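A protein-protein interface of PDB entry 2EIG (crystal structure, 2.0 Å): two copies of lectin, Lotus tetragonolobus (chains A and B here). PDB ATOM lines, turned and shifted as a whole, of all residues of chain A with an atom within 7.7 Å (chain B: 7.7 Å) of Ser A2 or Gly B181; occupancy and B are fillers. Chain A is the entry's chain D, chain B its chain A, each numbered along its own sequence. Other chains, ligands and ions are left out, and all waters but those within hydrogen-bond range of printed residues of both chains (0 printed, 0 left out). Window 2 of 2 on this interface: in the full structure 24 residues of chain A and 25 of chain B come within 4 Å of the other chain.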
ATOM      1  N   VAL A   1      -0.688   3.805 -13.217  1.00  0.00           N
ATOM      2  CA  VAL A   1      -1.149   5.077 -12.567  1.00  0.00           C
ATOM      3  C   VAL A   1      -0.254   6.164 -13.112  1.00  0.00           C
ATOM      4  O   VAL A   1       0.960   6.017 -13.135  1.00  0.00           O
ATOM      5  CB  VAL A   1      -1.093   5.031 -10.985  1.00  0.00           C
ATOM      6  CG1 VAL A   1      -1.283   6.387 -10.365  1.00  0.00           C
ATOM      7  CG2 VAL A   1      -2.153   4.094 -10.450  1.00  0.00           C
ATOM      8  N   SER A   2      -0.863   7.243 -13.583  1.00  0.00           N
ATOM      9  CA  SER A   2      -0.103   8.338 -14.181  1.00  0.00           C
ATOM     10  C   SER A   2      -0.687   9.649 -13.703  1.00  0.00           C
ATOM     11  O   SER A   2      -1.872   9.931 -13.926  1.00  0.00           O
ATOM     12  CB  SER A   2      -0.146   8.245 -15.730  1.00  0.00           C
ATOM     13  OG  SER A   2       0.286   9.454 -16.348  1.00  0.00           O
ATOM     14  N   PHE A   3       0.143  10.473 -13.081  1.00  0.00           N
ATOM     15  CA  PHE A   3      -0.255  11.824 -12.743  1.00  0.00           C
ATOM     16  C   PHE A   3       0.919  12.791 -12.811  1.00  0.00           C
ATOM     17  O   PHE A   3       2.065  12.369 -12.857  1.00  0.00           O
ATOM     18  CB  PHE A   3      -0.984  11.892 -11.389  1.00  0.00           C
ATOM     19  CG  PHE A   3      -0.183  11.383 -10.204  1.00  0.00           C
ATOM     20  CD1 PHE A   3       0.675  12.234  -9.511  1.00  0.00           C
ATOM     21  CD2 PHE A   3      -0.350  10.080  -9.744  1.00  0.00           C
ATOM     22  CE1 PHE A   3       1.375  11.775  -8.390  1.00  0.00           C
ATOM     23  CE2 PHE A   3       0.335   9.612  -8.642  1.00  0.00           C
ATOM     24  CZ  PHE A   3       1.209  10.491  -7.953  1.00  0.00           C
ATOM     25  N   ASN A   4       0.602  14.080 -12.820  1.00  0.00           N
ATOM     26  CA  ASN A   4       1.535  15.167 -13.086  1.00  0.00           C
ATOM     27  C   ASN A   4       0.970  16.440 -12.460  1.00  0.00           C
ATOM     28  O   ASN A   4       0.107  17.108 -13.051  1.00  0.00           O
ATOM     29  CB  ASN A   4       1.700  15.354 -14.610  1.00  0.00           C
ATOM     30  CG  ASN A   4       2.852  16.324 -14.998  1.00  0.00           C
ATOM     31  OD1 ASN A   4       3.661  16.787 -14.153  1.00  0.00           O
ATOM     32  ND2 ASN A   4       2.927  16.631 -16.305  1.00  0.00           N
ATOM     33  N   TYR A   5       1.436  16.759 -11.255  1.00  0.00           N
ATOM     34  CA  TYR A   5       1.168  18.062 -10.645  1.00  0.00           C
ATOM     35  C   TYR A   5       2.315  18.995 -10.951  1.00  0.00           C
ATOM     36  O   TYR A   5       3.444  18.782 -10.492  1.00  0.00           O
ATOM     37  CB  TYR A   5       0.993  17.939  -9.125  1.00  0.00           C
ATOM     38  CG  TYR A   5      -0.087  16.960  -8.758  1.00  0.00           C
ATOM     39  CD1 TYR A   5      -1.353  17.400  -8.350  1.00  0.00           C
ATOM     40  CD2 TYR A   5       0.150  15.594  -8.822  1.00  0.00           C
ATOM     41  CE1 TYR A   5      -2.355  16.496  -8.024  1.00  0.00           C
ATOM     42  CE2 TYR A   5      -0.834  14.687  -8.508  1.00  0.00           C
ATOM     43  CZ  TYR A   5      -2.079  15.135  -8.116  1.00  0.00           C
ATOM     44  OH  TYR A   5      -3.008  14.199  -7.821  1.00  0.00           O
ATOM     45  N   TYR A  45      -1.454  10.375  -2.822  1.00  0.00           N
ATOM     46  CA  TYR A  45      -2.285  10.405  -3.983  1.00  0.00           C
ATOM     47  C   TYR A  45      -3.562   9.598  -3.604  1.00  0.00           C
ATOM     48  O   TYR A  45      -3.471   8.532  -2.949  1.00  0.00           O
ATOM     49  CB  TYR A  45      -1.543   9.776  -5.158  1.00  0.00           C
ATOM     50  CG  TYR A  45      -2.337   9.732  -6.444  1.00  0.00           C
ATOM     51  CD1 TYR A  45      -2.648  10.907  -7.135  1.00  0.00           C
ATOM     52  CD2 TYR A  45      -2.748   8.517  -6.982  1.00  0.00           C
ATOM     53  CE1 TYR A  45      -3.359  10.860  -8.280  1.00  0.00           C
ATOM     54  CE2 TYR A  45      -3.446   8.469  -8.139  1.00  0.00           C
ATOM     55  CZ  TYR A  45      -3.744   9.640  -8.790  1.00  0.00           C
ATOM     56  OH  TYR A  45      -4.445   9.600  -9.972  1.00  0.00           O
ATOM     57  N   VAL A  49      -2.187   2.584  -5.570  1.00  0.00           N
ATOM     58  CA  VAL A  49      -1.385   2.193  -6.697  1.00  0.00           C
ATOM     59  C   VAL A  49      -1.158   0.698  -6.650  1.00  0.00           C
ATOM     60  O   VAL A  49      -0.536   0.184  -5.700  1.00  0.00           O
ATOM     61  CB  VAL A  49      -0.069   2.983  -6.748  1.00  0.00           C
ATOM     62  CG1 VAL A  49       0.808   2.463  -7.873  1.00  0.00           C
ATOM     63  CG2 VAL A  49      -0.356   4.472  -6.927  1.00  0.00           C
ATOM     64  N   SER A 222       5.337  14.303 -10.231  1.00  0.00           N
ATOM     65  CA  SER A 222       4.840  13.492 -11.334  1.00  0.00           C
ATOM     66  C   SER A 222       5.060  12.044 -10.961  1.00  0.00           C
ATOM     67  O   SER A 222       6.002  11.730 -10.249  1.00  0.00           O
ATOM     68  CB  SER A 222       5.584  13.824 -12.653  1.00  0.00           C
ATOM     69  OG  SER A 222       6.990  13.677 -12.536  1.00  0.00           O
ATOM     70  N   PHE A 223       4.206  11.155 -11.450  1.00  0.00           N
ATOM     71  CA  PHE A 223       4.337   9.756 -11.091  1.00  0.00           C
ATOM     72  C   PHE A 223       3.815   8.915 -12.234  1.00  0.00           C
ATOM     73  O   PHE A 223       2.766   9.218 -12.802  1.00  0.00           O
ATOM     74  CB  PHE A 223       3.570   9.451  -9.791  1.00  0.00           C
ATOM     75  CG  PHE A 223       3.619   8.009  -9.379  1.00  0.00           C
ATOM     76  CD1 PHE A 223       4.587   7.571  -8.471  1.00  0.00           C
ATOM     77  CD2 PHE A 223       2.684   7.087  -9.873  1.00  0.00           C
ATOM     78  CE1 PHE A 223       4.650   6.200  -8.070  1.00  0.00           C
ATOM     79  CE2 PHE A 223       2.744   5.736  -9.514  1.00  0.00           C
ATOM     80  CZ  PHE A 223       3.730   5.285  -8.615  1.00  0.00           C
ATOM     81  N   THR A 224       4.529   7.851 -12.568  1.00  0.00           N
ATOM     82  CA  THR A 224       4.056   6.916 -13.576  1.00  0.00           C
ATOM     83  C   THR A 224       4.372   5.533 -13.108  1.00  0.00           C
ATOM     84  O   THR A 224       5.540   5.230 -12.860  1.00  0.00           O
ATOM     85  CB  THR A 224       4.716   7.181 -14.959  1.00  0.00           C
ATOM     86  OG1 THR A 224       4.445   8.526 -15.299  1.00  0.00           O
ATOM     87  CG2 THR A 224       4.128   6.260 -16.090  1.00  0.00           C
ATOM     88  N   SER A 225       3.337   4.696 -12.969  1.00  0.00           N
ATOM     89  CA  SER A 225       3.548   3.283 -12.692  1.00  0.00           C
ATOM     90  C   SER A 225       2.892   2.417 -13.746  1.00  0.00           C
ATOM     91  O   SER A 225       1.902   2.818 -14.402  1.00  0.00           O
ATOM     92  CB  SER A 225       3.068   2.876 -11.289  1.00  0.00           C
ATOM     93  OG  SER A 225       1.676   3.052 -11.147  1.00  0.00           O
ATOM     94  N   THR A 226       3.472   1.245 -13.939  1.00  0.00           N
ATOM     95  CA  THR A 226       2.926   0.220 -14.847  1.00  0.00           C
ATOM     96  C   THR A 226       3.105  -1.137 -14.220  1.00  0.00           C
ATOM     97  O   THR A 226       4.221  -1.547 -13.889  1.00  0.00           O
ATOM     98  CB  THR A 226       3.563   0.242 -16.271  1.00  0.00           C
ATOM     99  OG1 THR A 226       3.362   1.534 -16.835  1.00  0.00           O
ATOM    100  CG2 THR A 226       2.890  -0.781 -17.173  1.00  0.00           C
ATOM    101  N   LEU B 158       5.747  10.852 -28.270  1.00  0.00           N
ATOM    102  CA  LEU B 158       6.787  11.401 -27.413  1.00  0.00           C
ATOM    103  C   LEU B 158       7.151  10.380 -26.372  1.00  0.00           C
ATOM    104  O   LEU B 158       6.283   9.800 -25.719  1.00  0.00           O
ATOM    105  CB  LEU B 158       6.344  12.696 -26.746  1.00  0.00           C
ATOM    106  CG  LEU B 158       7.345  13.284 -25.752  1.00  0.00           C
ATOM    107  CD1 LEU B 158       8.339  14.089 -26.559  1.00  0.00           C
ATOM    108  CD2 LEU B 158       6.580  14.138 -24.673  1.00  0.00           C
ATOM    109  N   MET B 176      11.413   4.873 -19.184  1.00  0.00           N
ATOM    110  CA  MET B 176      10.803   5.630 -20.313  1.00  0.00           C
ATOM    111  C   MET B 176       9.334   5.685 -20.104  1.00  0.00           C
ATOM    112  O   MET B 176       8.673   4.637 -20.091  1.00  0.00           O
ATOM    113  CB  MET B 176      10.867   4.931 -21.675  1.00  0.00           C
ATOM    114  CG  MET B 176      11.997   5.144 -22.451  1.00  0.00           C
ATOM    115  SD  MET B 176      13.209   4.219 -21.528  1.00  0.00           S
ATOM    116  CE  MET B 176      12.499   2.571 -21.313  1.00  0.00           C
ATOM    117  N   THR B 177       8.841   6.901 -19.960  1.00  0.00           N
ATOM    118  CA  THR B 177       7.449   7.191 -19.765  1.00  0.00           C
ATOM    119  C   THR B 177       6.943   7.446 -21.188  1.00  0.00           C
ATOM    120  O   THR B 177       7.471   8.289 -21.957  1.00  0.00           O
ATOM    121  CB  THR B 177       7.298   8.408 -18.845  1.00  0.00           C
ATOM    122  OG1 THR B 177       7.907   8.099 -17.574  1.00  0.00           O
ATOM    123  CG2 THR B 177       5.778   8.834 -18.637  1.00  0.00           C
ATOM    124  N   HIS B 178       5.935   6.679 -21.539  1.00  0.00           N
ATOM    125  CA  HIS B 178       5.338   6.778 -22.843  1.00  0.00           C
ATOM    126  C   HIS B 178       4.119   7.667 -22.799  1.00  0.00           C
ATOM    127  O   HIS B 178       3.530   7.907 -21.711  1.00  0.00           O
ATOM    128  CB  HIS B 178       5.021   5.370 -23.322  1.00  0.00           C
ATOM    129  CG  HIS B 178       6.130   4.413 -23.058  1.00  0.00           C
ATOM    130  ND1 HIS B 178       5.988   3.304 -22.239  1.00  0.00           N
ATOM    131  CD2 HIS B 178       7.424   4.425 -23.461  1.00  0.00           C
ATOM    132  CE1 HIS B 178       7.136   2.651 -22.194  1.00  0.00           C
ATOM    133  NE2 HIS B 178       8.025   3.315 -22.925  1.00  0.00           N
ATOM    134  N   GLN B 179       3.761   8.143 -23.990  1.00  0.00           N
ATOM    135  CA  GLN B 179       2.629   9.053 -24.211  1.00  0.00           C
ATOM    136  C   GLN B 179       1.317   8.523 -23.614  1.00  0.00           C
ATOM    137  O   GLN B 179       0.492   9.293 -23.118  1.00  0.00           O
ATOM    138  CB  GLN B 179       2.484   9.311 -25.727  1.00  0.00           C
ATOM    139  CG  GLN B 179       1.315  10.161 -26.158  1.00  0.00           C
ATOM    140  CD  GLN B 179       1.616  11.651 -26.065  1.00  0.00           C
ATOM    141  OE1 GLN B 179       2.621  12.059 -25.473  1.00  0.00           O
ATOM    142  NE2 GLN B 179       0.731  12.477 -26.650  1.00  0.00           N
ATOM    143  N   ASN B 180       1.137   7.208 -23.652  1.00  0.00           N
ATOM    144  CA  ASN B 180      -0.052   6.590 -23.084  1.00  0.00           C
ATOM    145  C   ASN B 180      -0.057   6.534 -21.541  1.00  0.00           C
ATOM    146  O   ASN B 180      -0.977   5.971 -20.927  1.00  0.00           O
ATOM    147  CB  ASN B 180      -0.262   5.216 -23.716  1.00  0.00           C
ATOM    148  CG  ASN B 180       0.677   4.133 -23.156  1.00  0.00           C
ATOM    149  OD1 ASN B 180       0.464   2.940 -23.430  1.00  0.00           O
ATOM    150  ND2 ASN B 180       1.710   4.528 -22.398  1.00  0.00           N
ATOM    151  N   GLY B 181       0.963   7.113 -20.894  1.00  0.00           N
ATOM    152  CA  GLY B 181       0.966   7.142 -19.432  1.00  0.00           C
ATOM    153  C   GLY B 181       1.512   5.875 -18.765  1.00  0.00           C
ATOM    154  O   GLY B 181       1.410   5.721 -17.550  1.00  0.00           O
ATOM    155  N   GLN B 182       2.043   4.959 -19.569  1.00  0.00           N
ATOM    156  CA  GLN B 182       2.736   3.771 -19.101  1.00  0.00           C
ATOM    157  C   GLN B 182       4.242   4.084 -18.977  1.00  0.00           C
ATOM    158  O   GLN B 182       4.705   5.079 -19.528  1.00  0.00           O
ATOM    159  CB  GLN B 182       2.504   2.572 -20.053  1.00  0.00           C
ATOM    160  CG  GLN B 182       1.048   2.062 -20.167  1.00  0.00           C
ATOM    161  CD  GLN B 182       0.980   0.591 -20.613  1.00  0.00           C
ATOM    162  OE1 GLN B 182       1.977  -0.137 -20.592  1.00  0.00           O
ATOM    163  NE2 GLN B 182      -0.209   0.152 -21.003  1.00  0.00           N
ATOM    164  N   ILE B 183       4.992   3.278 -18.227  1.00  0.00           N
ATOM    165  CA  ILE B 183       6.461   3.388 -18.225  1.00  0.00           C
ATOM    166  C   ILE B 183       7.051   2.015 -18.444  1.00  0.00           C
ATOM    167  O   ILE B 183       6.444   1.014 -18.093  1.00  0.00           O
ATOM    168  CB  ILE B 183       7.113   3.761 -16.852  1.00  0.00           C
ATOM    169  CG1 ILE B 183       6.130   3.807 -15.719  1.00  0.00           C
ATOM    170  CG2 ILE B 183       8.194   4.723 -16.948  1.00  0.00           C
ATOM    171  CD1 ILE B 183       6.168   2.464 -15.122  1.00  0.00           C
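No position is printed for both chains.
The backbone NH (N) of Gln B182 lies close to the side-chain amide nitrogen (ND2) of Asn B180, at 2.9 Å.
The backbone carbonyl oxygen of Gln B182 lies within hydrogen-bond range of a ring nitrogen (ND1) of His B178, at 3.5 Å.
The backbone carbonyl oxygen (O) of Val A1 lies within hydrogen-bond range of the backbone NH (N) of Ser A225 (2.7 Å).
Ser A2 touches just one residue of chain B: Gly B181 (3.5 Å).
Phe A3 touches none of the printed residues of chain B.
Printed residues of chain B within 4 Å of Ser A225: Ile B183 (3.6 Å).
Of the printed residues of chain B, Thr A226 touches Gln B182 and Ile B183.
Of chain A, only Ser A2 and Thr A224 come within 4 Å of Gly B181.
Of the printed residues of chain A, Gln B182 touches Thr A224 and Thr A226.
The nearest residue of chain A that does not touch Gly B181 is Ser A225 (4.3 Å).
Among the printed residues, pairs that only touch across the chains: Ser A2 with Gly B181 (3.5 Å), Thr A224 with Thr B177 (3.6 Å), Thr A224 with Gly B181 (3.1 Å), Thr A224 with Gln B182 (3.6 Å), Thr A224 with Ile B183 (3.2 Å), Ser A225 with Ile B183 (3.6 Å) and Thr A226 with Gln B182 (3.2 Å).
The backbone NH of Ile B183 sits at hydrogen-bond distance from the side-chain hydroxyl of Thr A226 (2.8 Å).
Of the 9 printed residues of chain B, 4 touch a printed residue of chain A.
Hydrophobic or aromatic side chains of chain B within 4 Å of the printed part of chain A: Ile B183.
Along chain B the printed residues that touch a printed residue of chain A span positions 177 to 183.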
